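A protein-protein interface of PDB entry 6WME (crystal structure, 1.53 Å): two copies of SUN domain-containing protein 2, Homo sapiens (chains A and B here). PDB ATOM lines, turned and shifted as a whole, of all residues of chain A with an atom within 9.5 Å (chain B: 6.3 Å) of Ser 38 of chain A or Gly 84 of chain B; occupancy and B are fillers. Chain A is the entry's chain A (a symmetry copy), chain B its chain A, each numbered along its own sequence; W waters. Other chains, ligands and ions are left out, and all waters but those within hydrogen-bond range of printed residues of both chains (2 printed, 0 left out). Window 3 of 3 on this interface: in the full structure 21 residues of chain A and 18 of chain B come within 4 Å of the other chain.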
ATOM      1  N   ASP A  27      10.097  14.217 -21.498  1.00  0.00           N
ATOM      2  CA  ASP A  27      10.563  14.226 -22.896  1.00  0.00           C
ATOM      3  C   ASP A  27       9.412  13.874 -23.851  1.00  0.00           C
ATOM      4  O   ASP A  27       9.612  13.209 -24.867  1.00  0.00           O
ATOM      5  CB  ASP A  27      11.757  13.264 -23.062  1.00  0.00           C
ATOM      6  CG  ASP A  27      12.723  13.651 -24.191  1.00  0.00           C
ATOM      7  OD1 ASP A  27      12.620  14.754 -24.783  1.00  0.00           O
ATOM      8  OD2 ASP A  27      13.616  12.811 -24.479  1.00  0.00           O
ATOM      9  N   ASP A  33      15.987   7.770 -23.833  1.00  0.00           N
ATOM     10  CA  ASP A  33      16.587   7.969 -25.154  1.00  0.00           C
ATOM     11  C   ASP A  33      18.094   7.733 -25.071  1.00  0.00           C
ATOM     12  O   ASP A  33      18.842   8.594 -24.585  1.00  0.00           O
ATOM     13  CB  ASP A  33      16.284   9.374 -25.682  1.00  0.00           C
ATOM     14  CG  ASP A  33      16.960   9.669 -27.028  1.00  0.00           C
ATOM     15  OD1 ASP A  33      17.441   8.733 -27.696  1.00  0.00           O
ATOM     16  OD2 ASP A  33      16.995  10.850 -27.436  1.00  0.00           O
ATOM     17  N   TYR A  34      18.543   6.600 -25.607  1.00  0.00           N
ATOM     18  CA  TYR A  34      19.960   6.258 -25.622  1.00  0.00           C
ATOM     19  C   TYR A  34      20.733   6.965 -26.730  1.00  0.00           C
ATOM     20  O   TYR A  34      21.959   6.807 -26.819  1.00  0.00           O
ATOM     21  CB  TYR A  34      20.111   4.736 -25.733  1.00  0.00           C
ATOM     22  CG  TYR A  34      19.553   4.051 -24.517  1.00  0.00           C
ATOM     23  CD1 TYR A  34      20.332   3.838 -23.389  1.00  0.00           C
ATOM     24  CD2 TYR A  34      18.220   3.675 -24.473  1.00  0.00           C
ATOM     25  CE1 TYR A  34      19.798   3.237 -22.249  1.00  0.00           C
ATOM     26  CE2 TYR A  34      17.674   3.075 -23.343  1.00  0.00           C
ATOM     27  CZ  TYR A  34      18.470   2.856 -22.239  1.00  0.00           C
ATOM     28  OH  TYR A  34      17.927   2.266 -21.116  1.00  0.00           O
ATOM     29  N   ALA A  35      20.064   7.760 -27.563  1.00  0.00           N
ATOM     30  CA  ALA A  35      20.739   8.604 -28.542  1.00  0.00           C
ATOM     31  C   ALA A  35      20.870  10.058 -28.092  1.00  0.00           C
ATOM     32  O   ALA A  35      21.428  10.881 -28.836  1.00  0.00           O
ATOM     33  CB  ALA A  35      20.007   8.535 -29.887  1.00  0.00           C
ATOM     34  N   LEU A  36      20.414  10.397 -26.887  1.00  0.00           N
ATOM     35  CA  LEU A  36      20.533  11.766 -26.402  1.00  0.00           C
ATOM     36  C   LEU A  36      21.993  12.123 -26.114  1.00  0.00           C
ATOM     37  O   LEU A  36      22.664  11.441 -25.334  1.00  0.00           O
ATOM     38  CB  LEU A  36      19.692  11.932 -25.142  1.00  0.00           C
ATOM     39  CG  LEU A  36      19.538  13.352 -24.616  1.00  0.00           C
ATOM     40  CD1 LEU A  36      18.771  14.219 -25.604  1.00  0.00           C
ATOM     41  CD2 LEU A  36      18.859  13.299 -23.242  1.00  0.00           C
ATOM     42  N   GLU A  37      22.482  13.225 -26.707  1.00  0.00           N
ATOM     43  CA  GLU A  37      23.903  13.545 -26.563  1.00  0.00           C
ATOM     44  C   GLU A  37      24.282  13.785 -25.106  1.00  0.00           C
ATOM     45  O   GLU A  37      25.308  13.278 -24.640  1.00  0.00           O
ATOM     46  CB  GLU A  37      24.261  14.757 -27.417  1.00  0.00           C
ATOM     47  CG  GLU A  37      25.770  15.000 -27.476  1.00  0.00           C
ATOM     48  CD  GLU A  37      26.160  16.165 -28.393  1.00  0.00           C
ATOM     49  OE1 GLU A  37      25.786  17.309 -28.062  1.00  0.00           O
ATOM     50  OE2 GLU A  37      26.834  15.918 -29.419  1.00  0.00           O
ATOM     51  N   SER A  38      23.453  14.526 -24.353  1.00  0.00           N
ATOM     52  CA  SER A  38      23.830  14.843 -22.978  1.00  0.00           C
ATOM     53  C   SER A  38      23.873  13.606 -22.093  1.00  0.00           C
ATOM     54  O   SER A  38      24.585  13.609 -21.081  1.00  0.00           O
ATOM     55  CB  SER A  38      22.889  15.903 -22.389  1.00  0.00           C
ATOM     56  OG  SER A  38      21.550  15.432 -22.327  1.00  0.00           O
ATOM     57  N   GLY A  39      23.142  12.554 -22.455  1.00  0.00           N
ATOM     58  CA  GLY A  39      23.214  11.295 -21.736  1.00  0.00           C
ATOM     59  C   GLY A  39      24.395  10.422 -22.100  1.00  0.00           C
ATOM     60  O   GLY A  39      24.559   9.352 -21.498  1.00  0.00           O
ATOM     61  N   GLY A  40      25.221  10.839 -23.075  1.00  0.00           N
ATOM     62  CA  GLY A  40      26.371  10.041 -23.458  1.00  0.00           C
ATOM     63  C   GLY A  40      26.424   9.542 -24.888  1.00  0.00           C
ATOM     64  O   GLY A  40      27.308   8.744 -25.223  1.00  0.00           O
ATOM     65  N   ALA A  41      25.501   9.975 -25.743  1.00  0.00           N
ATOM     66  CA  ALA A  41      25.544   9.551 -27.137  1.00  0.00           C
ATOM     67  C   ALA A  41      26.379  10.528 -27.960  1.00  0.00           C
ATOM     68  O   ALA A  41      26.560  11.696 -27.592  1.00  0.00           O
ATOM     69  CB  ALA A  41      24.129   9.452 -27.715  1.00  0.00           C
ATOM     70  N   SER A  42      26.893  10.043 -29.089  1.00  0.00           N
ATOM     71  CA  SER A  42      27.648  10.943 -29.953  1.00  0.00           C
ATOM     72  C   SER A  42      27.590  10.453 -31.393  1.00  0.00           C
ATOM     73  O   SER A  42      27.366   9.269 -31.651  1.00  0.00           O
ATOM     74  CB  SER A  42      29.112  11.088 -29.501  1.00  0.00           C
ATOM     75  OG  SER A  42      29.708   9.833 -29.221  1.00  0.00           O
ATOM     76  N   ARG A  74      25.614  16.632 -34.826  1.00  0.00           N
ATOM     77  CA  ARG A  74      25.341  16.588 -33.387  1.00  0.00           C
ATOM     78  C   ARG A  74      23.939  17.059 -33.057  1.00  0.00           C
ATOM     79  O   ARG A  74      23.351  16.614 -32.058  1.00  0.00           O
ATOM     80  CB  ARG A  74      26.315  17.485 -32.615  1.00  0.00           C
ATOM     81  CG  ARG A  74      27.765  17.044 -32.622  1.00  0.00           C
ATOM     82  CD  ARG A  74      28.656  18.036 -31.834  1.00  0.00           C
ATOM     83  NE  ARG A  74      28.199  18.174 -30.453  1.00  0.00           N
ATOM     84  CZ  ARG A  74      28.706  19.030 -29.576  1.00  0.00           C
ATOM     85  NH1 ARG A  74      29.699  19.845 -29.929  1.00  0.00           N
ATOM     86  NH2 ARG A  74      28.230  19.087 -28.343  1.00  0.00           N
ATOM     87  N   ILE A  76      21.070  16.467 -34.231  1.00  0.00           N
ATOM     88  CA  ILE A  76      19.989  15.473 -34.217  1.00  0.00           C
ATOM     89  C   ILE A  76      19.890  14.721 -32.896  1.00  0.00           C
ATOM     90  O   ILE A  76      18.884  14.035 -32.650  1.00  0.00           O
ATOM     91  CB  ILE A  76      20.078  14.456 -35.376  1.00  0.00           C
ATOM     92  CG1 ILE A  76      21.131  13.373 -35.126  1.00  0.00           C
ATOM     93  CG2 ILE A  76      20.333  15.165 -36.713  1.00  0.00           C
ATOM     94  CD1 ILE A  76      21.148  12.293 -36.240  1.00  0.00           C
ATOM     95  N   LEU A  77      20.888  14.866 -32.030  1.00  0.00           N
ATOM     96  CA  LEU A  77      20.925  14.265 -30.706  1.00  0.00           C
ATOM     97  C   LEU A  77      20.646  15.285 -29.615  1.00  0.00           C
ATOM     98  O   LEU A  77      20.939  15.030 -28.438  1.00  0.00           O
ATOM     99  CB  LEU A  77      22.292  13.600 -30.483  1.00  0.00           C
ATOM    100  CG  LEU A  77      22.805  12.710 -31.610  1.00  0.00           C
ATOM    101  CD1 LEU A  77      24.127  12.114 -31.197  1.00  0.00           C
ATOM    102  CD2 LEU A  77      21.810  11.600 -31.941  1.00  0.00           C
ATOM    103  N   GLN A  78      20.068  16.435 -29.977  1.00  0.00           N
ATOM    104  CA  GLN A  78      19.870  17.524 -29.038  1.00  0.00           C
ATOM    105  C   GLN A  78      18.384  17.905 -29.023  1.00  0.00           C
ATOM    106  O   GLN A  78      17.719  17.826 -30.058  1.00  0.00           O
ATOM    107  CB  GLN A  78      20.749  18.732 -29.422  1.00  0.00           C
ATOM    108  CG  GLN A  78      22.263  18.413 -29.348  1.00  0.00           C
ATOM    109  CD  GLN A  78      23.160  19.535 -29.873  1.00  0.00           C
ATOM    110  OE1 GLN A  78      22.680  20.526 -30.433  1.00  0.00           O
ATOM    111  NE2 GLN A  78      24.460  19.384 -29.674  1.00  0.00           N
ATOM    112  N   PRO A  79      17.852  18.255 -27.851  1.00  0.00           N
ATOM    113  CA  PRO A  79      16.385  18.364 -27.721  1.00  0.00           C
ATOM    114  C   PRO A  79      15.749  19.621 -28.280  1.00  0.00           C
ATOM    115  O   PRO A  79      14.530  19.589 -28.535  1.00  0.00           O
ATOM    116  CB  PRO A  79      16.161  18.294 -26.198  1.00  0.00           C
ATOM    117  CG  PRO A  79      17.454  18.780 -25.607  1.00  0.00           C
ATOM    118  CD  PRO A  79      18.541  18.297 -26.554  1.00  0.00           C
ATOM    119  N   ARG A  99      26.911   6.541 -32.001  1.00  0.00           N
ATOM    120  CA  ARG A  99      27.298   5.692 -30.882  1.00  0.00           C
ATOM    121  C   ARG A  99      26.372   6.013 -29.715  1.00  0.00           C
ATOM    122  O   ARG A  99      26.452   7.101 -29.132  1.00  0.00           O
ATOM    123  CB  ARG A  99      28.759   5.911 -30.499  1.00  0.00           C
ATOM    124  CG  ARG A  99      29.236   5.046 -29.342  1.00  0.00           C
ATOM    125  CD  ARG A  99      30.633   5.484 -28.861  1.00  0.00           C
ATOM    126  NE  ARG A  99      31.141   4.633 -27.781  1.00  0.00           N
ATOM    127  CZ  ARG A  99      30.796   4.754 -26.499  1.00  0.00           C
ATOM    128  NH1 ARG A  99      31.314   3.929 -25.597  1.00  0.00           N
ATOM    129  NH2 ARG A  99      29.925   5.688 -26.114  1.00  0.00           N
ATOM    130  N   SER A 101      24.572   5.835 -25.935  1.00  0.00           N
ATOM    131  CA  SER A 101      25.217   6.034 -24.641  1.00  0.00           C
ATOM    132  C   SER A 101      25.502   4.720 -23.930  1.00  0.00           C
ATOM    133  O   SER A 101      26.394   4.673 -23.075  1.00  0.00           O
ATOM    134  CB  SER A 101      24.361   6.935 -23.749  1.00  0.00           C
ATOM    135  OG  SER A 101      23.046   6.401 -23.542  1.00  0.00           O
ATOM    136  N   ARG A 193      15.331  15.757 -34.769  1.00  0.00           N
ATOM    137  CA  ARG A 193      15.845  14.956 -33.663  1.00  0.00           C
ATOM    138  C   ARG A 193      15.516  13.484 -33.873  1.00  0.00           C
ATOM    139  O   ARG A 193      14.394  13.129 -34.262  1.00  0.00           O
ATOM    140  CB  ARG A 193      15.291  15.418 -32.302  1.00  0.00           C
ATOM    141  CG  ARG A 193      15.801  14.562 -31.129  1.00  0.00           C
ATOM    142  CD  ARG A 193      15.351  15.078 -29.755  1.00  0.00           C
ATOM    143  NE  ARG A 193      15.706  14.122 -28.713  1.00  0.00           N
ATOM    144  CZ  ARG A 193      15.110  14.050 -27.521  1.00  0.00           C
ATOM    145  NH1 ARG A 193      14.161  14.920 -27.187  1.00  0.00           N
ATOM    146  NH2 ARG A 193      15.472  13.105 -26.654  1.00  0.00           N
ATOM    147  N   GLN B  71      30.652  18.853 -16.422  1.00  0.00           N
ATOM    148  CA  GLN B  71      29.668  19.828 -15.970  1.00  0.00           C
ATOM    149  C   GLN B  71      30.134  20.463 -14.668  1.00  0.00           C
ATOM    150  O   GLN B  71      30.444  19.756 -13.709  1.00  0.00           O
ATOM    151  CB  GLN B  71      28.308  19.162 -15.768  1.00  0.00           C
ATOM    152  CG  GLN B  71      27.827  18.292 -16.923  1.00  0.00           C
ATOM    153  CD  GLN B  71      27.511  19.101 -18.153  1.00  0.00           C
ATOM    154  OE1 GLN B  71      27.131  20.265 -18.063  1.00  0.00           O
ATOM    155  NE2 GLN B  71      27.680  18.492 -19.320  1.00  0.00           N
ATOM    156  N   ASP B  80      17.895  23.681 -17.751  1.00  0.00           N
ATOM    157  CA  ASP B  80      17.894  22.471 -18.567  1.00  0.00           C
ATOM    158  C   ASP B  80      18.195  21.270 -17.673  1.00  0.00           C
ATOM    159  O   ASP B  80      19.255  21.222 -17.044  1.00  0.00           O
ATOM    160  CB  ASP B  80      18.939  22.618 -19.681  1.00  0.00           C
ATOM    161  CG  ASP B  80      18.930  21.470 -20.683  1.00  0.00           C
ATOM    162  OD1 ASP B  80      18.624  20.319 -20.312  1.00  0.00           O
ATOM    163  OD2 ASP B  80      19.270  21.726 -21.863  1.00  0.00           O
ATOM    164  N   VAL B  81      17.280  20.299 -17.613  1.00  0.00           N
ATOM    165  CA  VAL B  81      17.493  19.143 -16.741  1.00  0.00           C
ATOM    166  C   VAL B  81      17.337  17.833 -17.505  1.00  0.00           C
ATOM    167  O   VAL B  81      16.938  16.810 -16.929  1.00  0.00           O
ATOM    168  CB  VAL B  81      16.556  19.181 -15.521  1.00  0.00           C
ATOM    169  CG1 VAL B  81      17.027  20.266 -14.552  1.00  0.00           C
ATOM    170  CG2 VAL B  81      15.095  19.392 -15.959  1.00  0.00           C
ATOM    171  N   HIS B  82      17.676  17.844 -18.800  1.00  0.00           N
ATOM    172  CA  HIS B  82      17.743  16.595 -19.542  1.00  0.00           C
ATOM    173  C   HIS B  82      18.814  15.706 -18.918  1.00  0.00           C
ATOM    174  O   HIS B  82      19.742  16.209 -18.280  1.00  0.00           O
ATOM    175  CB  HIS B  82      18.062  16.861 -21.012  1.00  0.00           C
ATOM    176  CG  HIS B  82      16.926  17.474 -21.769  1.00  0.00           C
ATOM    177  ND1 HIS B  82      16.776  18.837 -21.913  1.00  0.00           N
ATOM    178  CD2 HIS B  82      15.902  16.908 -22.443  1.00  0.00           C
ATOM    179  CE1 HIS B  82      15.690  19.082 -22.626  1.00  0.00           C
ATOM    180  NE2 HIS B  82      15.140  17.928 -22.955  1.00  0.00           N
ATOM    181  N   PRO B  83      18.712  14.389 -19.093  1.00  0.00           N
ATOM    182  CA  PRO B  83      19.711  13.483 -18.505  1.00  0.00           C
ATOM    183  C   PRO B  83      21.142  13.914 -18.795  1.00  0.00           C
ATOM    184  O   PRO B  83      21.518  14.165 -19.947  1.00  0.00           O
ATOM    185  CB  PRO B  83      19.385  12.137 -19.158  1.00  0.00           C
ATOM    186  CG  PRO B  83      17.893  12.201 -19.377  1.00  0.00           C
ATOM    187  CD  PRO B  83      17.601  13.651 -19.729  1.00  0.00           C
ATOM    188  N   GLY B  84      21.950  13.983 -17.728  1.00  0.00           N
ATOM    189  CA  GLY B  84      23.343  14.374 -17.833  1.00  0.00           C
ATOM    190  C   GLY B  84      23.598  15.862 -17.696  1.00  0.00           C
ATOM    191  O   GLY B  84      24.768  16.265 -17.569  1.00  0.00           O
ATOM    192  N   ASN B  85      22.555  16.696 -17.732  1.00  0.00           N
ATOM    193  CA  ASN B  85      22.708  18.135 -17.494  1.00  0.00           C
ATOM    194  C   ASN B  85      22.626  18.387 -15.987  1.00  0.00           C
ATOM    195  O   ASN B  85      21.686  18.976 -15.455  1.00  0.00           O
ATOM    196  CB  ASN B  85      21.664  18.920 -18.277  1.00  0.00           C
ATOM    197  CG  ASN B  85      21.947  18.912 -19.762  1.00  0.00           C
ATOM    198  OD1 ASN B  85      23.072  18.654 -20.182  1.00  0.00           O
ATOM    199  ND2 ASN B  85      20.935  19.195 -20.562  1.00  0.00           N
ATOM    200  N   CYS B  86      23.640  17.866 -15.301  1.00  0.00           N
ATOM    201  CA  CYS B  86      23.711  17.792 -13.849  1.00  0.00           C
ATOM    202  C   CYS B  86      25.167  17.896 -13.429  1.00  0.00           C
ATOM    203  O   CYS B  86      26.068  17.516 -14.177  1.00  0.00           O
ATOM    204  CB  CYS B  86      23.076  16.506 -13.324  1.00  0.00           C
ATOM    205  SG  CYS B  86      23.740  14.998 -14.099  1.00  0.00           S
ATOM    206  N   TRP B  87      25.386  18.415 -12.225  1.00  0.00           N
ATOM    207  CA  TRP B  87      26.715  18.481 -11.636  1.00  0.00           C
ATOM    208  C   TRP B  87      26.939  17.249 -10.774  1.00  0.00           C
ATOM    209  O   TRP B  87      26.076  16.897  -9.963  1.00  0.00           O
ATOM    210  CB  TRP B  87      26.853  19.755 -10.801  1.00  0.00           C
ATOM    211  CG  TRP B  87      28.148  19.843 -10.032  1.00  0.00           C
ATOM    212  CD1 TRP B  87      29.423  19.838 -10.541  1.00  0.00           C
ATOM    213  CD2 TRP B  87      28.278  19.946  -8.611  1.00  0.00           C
ATOM    214  NE1 TRP B  87      30.337  19.929  -9.511  1.00  0.00           N
ATOM    215  CE2 TRP B  87      29.659  20.010  -8.321  1.00  0.00           C
ATOM    216  CE3 TRP B  87      27.362  20.008  -7.552  1.00  0.00           C
ATOM    217  CZ2 TRP B  87      30.144  20.115  -7.012  1.00  0.00           C
ATOM    218  CZ3 TRP B  87      27.844  20.118  -6.252  1.00  0.00           C
ATOM    219  CH2 TRP B  87      29.223  20.165  -5.994  1.00  0.00           C
ATOM    220  N   VAL B 114      16.275  13.872 -12.605  1.00  0.00           N
ATOM    221  CA  VAL B 114      15.695  13.334 -13.842  1.00  0.00           C
ATOM    222  C   VAL B 114      14.609  12.319 -13.480  1.00  0.00           C
ATOM    223  O   VAL B 114      14.737  11.611 -12.459  1.00  0.00           O
ATOM    224  CB  VAL B 114      16.807  12.707 -14.715  1.00  0.00           C
ATOM    225  CG1 VAL B 114      17.564  11.642 -13.947  1.00  0.00           C
ATOM    226  CG2 VAL B 114      16.271  12.160 -16.041  1.00  0.00           C
ATOM    227  N   TYR B 192      20.743  17.924 -10.359  1.00  0.00           N
ATOM    228  CA  TYR B 192      20.225  18.510 -11.600  1.00  0.00           C
ATOM    229  C   TYR B 192      19.895  19.993 -11.439  1.00  0.00           C
ATOM    230  O   TYR B 192      20.351  20.822 -12.233  1.00  0.00           O
ATOM    231  CB  TYR B 192      18.990  17.732 -12.104  1.00  0.00           C
ATOM    232  CG  TYR B 192      19.414  16.507 -12.880  1.00  0.00           C
ATOM    233  CD1 TYR B 192      19.829  15.351 -12.222  1.00  0.00           C
ATOM    234  CD2 TYR B 192      19.475  16.530 -14.262  1.00  0.00           C
ATOM    235  CE1 TYR B 192      20.266  14.233 -12.943  1.00  0.00           C
ATOM    236  CE2 TYR B 192      19.902  15.427 -14.985  1.00  0.00           C
ATOM    237  CZ  TYR B 192      20.300  14.287 -14.324  1.00  0.00           C
ATOM    238  OH  TYR B 192      20.733  13.198 -15.069  1.00  0.00           O
HETATM  239  O   HOH W   1      26.534  15.444 -20.296  1.00  0.00           O
HETATM  240  O   HOH W   2      12.554  17.354 -24.379  1.00  0.00           O
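The side-chain hydroxyl (OG) of Ser 38 of chain A is in hydrogen-bond range of the backbone carbonyl oxygen (O) of Pro 83 of chain B, 2.7 Å away. The backbone carbonyl oxygen of Pro 83 of chain B is in hydrogen-bond range of the backbone NH of Gly 39 of chain A.
OD1 of Asp 80 of chain B lies within hydrogen-bond range of ND1 of His 82 of chain B, 2.9 Å away. The side-chain carboxylate (OD1) of Asp 80 of chain B sits at hydrogen-bond distance from the side-chain amide nitrogen (ND2) of Asn 85 of chain B (2.6 Å). OH of Tyr 192 of chain B sits at hydrogen-bond distance from N of Gly 84 of chain B, at 3.0 Å. The side-chain carboxylate (OD2) of Asp 33 of chain A lies within hydrogen-bond range of the backbone NH (N) of Leu 36 of chain A. The backbone NH of Ala 41 of chain A sits at hydrogen-bond distance from the backbone carbonyl oxygen of Leu 36 of chain A, 3.2 Å away.
Pro 83 of chain B touches Leu 36 of chain A (CD to CD2, 3.7 Å). His 82 of chain B touches Ser 38 of chain A (CB to OG, 3.99 Å). O of Ser 38 of chain A touches CA of Gly 84 of chain B, 3.6 Å away. Asn 85 of chain B touches Ser 38 of chain A (OD1 to CB, 3.5 Å). Pro 79 of chain A touches His 82 of chain B (CB to NE2, 3.4 Å).
Printed residues of chain B within 4 Å of Leu 36 of chain A: Pro 83. Printed residues of chain B within 4 Å of Ser 38 of chain A: His 82 (3.99 Å), Pro 83 (2.7 Å), Gly 84 (3.6 Å) and Asn 85 (3.5 Å). Of the printed residues of chain B, Gly 39 of chain A touches Pro 83. Of the printed residues of chain B, Pro 79 of chain A touches His 82 (3.4 Å). Of the printed residues of chain A, His 82 of chain B touches Ser 38 and Pro 79. Of chain A, only Leu 36, Ser 38 and Gly 39 come within 4 Å of Pro 83 of chain B. Gly 84 of chain B touches one residue of chain A. Asn 85 of chain B touches just one residue of chain A: Ser 38 (3.5 Å). The nearest residue of chain A that does not touch Gly 84 of chain B is Gly 39 of chain A (5.0 Å). The nearest printed residue of chain A that does not touch His 82 of chain B is Leu 36 of chain A (4.3 Å).
Of the 11 printed residues of chain B, 4 touch a printed residue of chain A. Printed residues of chain B that touch a printed residue of chain A: His 82, Pro 83, Gly 84 and Asn 85. Hydrophobic or aromatic side chains of chain B within 4 Å of the printed part of chain A: His 82 and Pro 83. Of the 19 printed residues of chain A, 4 touch a printed residue of chain B. Printed residues of chain A that touch a printed residue of chain B: Leu 36, Ser 38, Gly 39 and Pro 79. Hydrophobic or aromatic side chains of chain A that line the printed part of chain B: Leu 36 and Pro 79. Among the printed residues, 7 pairs touch across the chains. Among the printed residues, no Asp or Glu carboxylate lies within 4 Å of a Lys or Arg side-chain nitrogen of the other chain.
No position is printed for both chains.
Water W2 bridges the side-chain carboxylate of Asp 27 of chain A (2.6 Å) and a ring nitrogen (NE2) of His 82 of chain B (3.0 Å). Water W1 lies within hydrogen-bond range of O of Ser 38 of chain A (2.8 Å), O of Gly 84 of chain B (3.4 Å) and NE2 of Gln 71 of chain B (3.4 Å).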
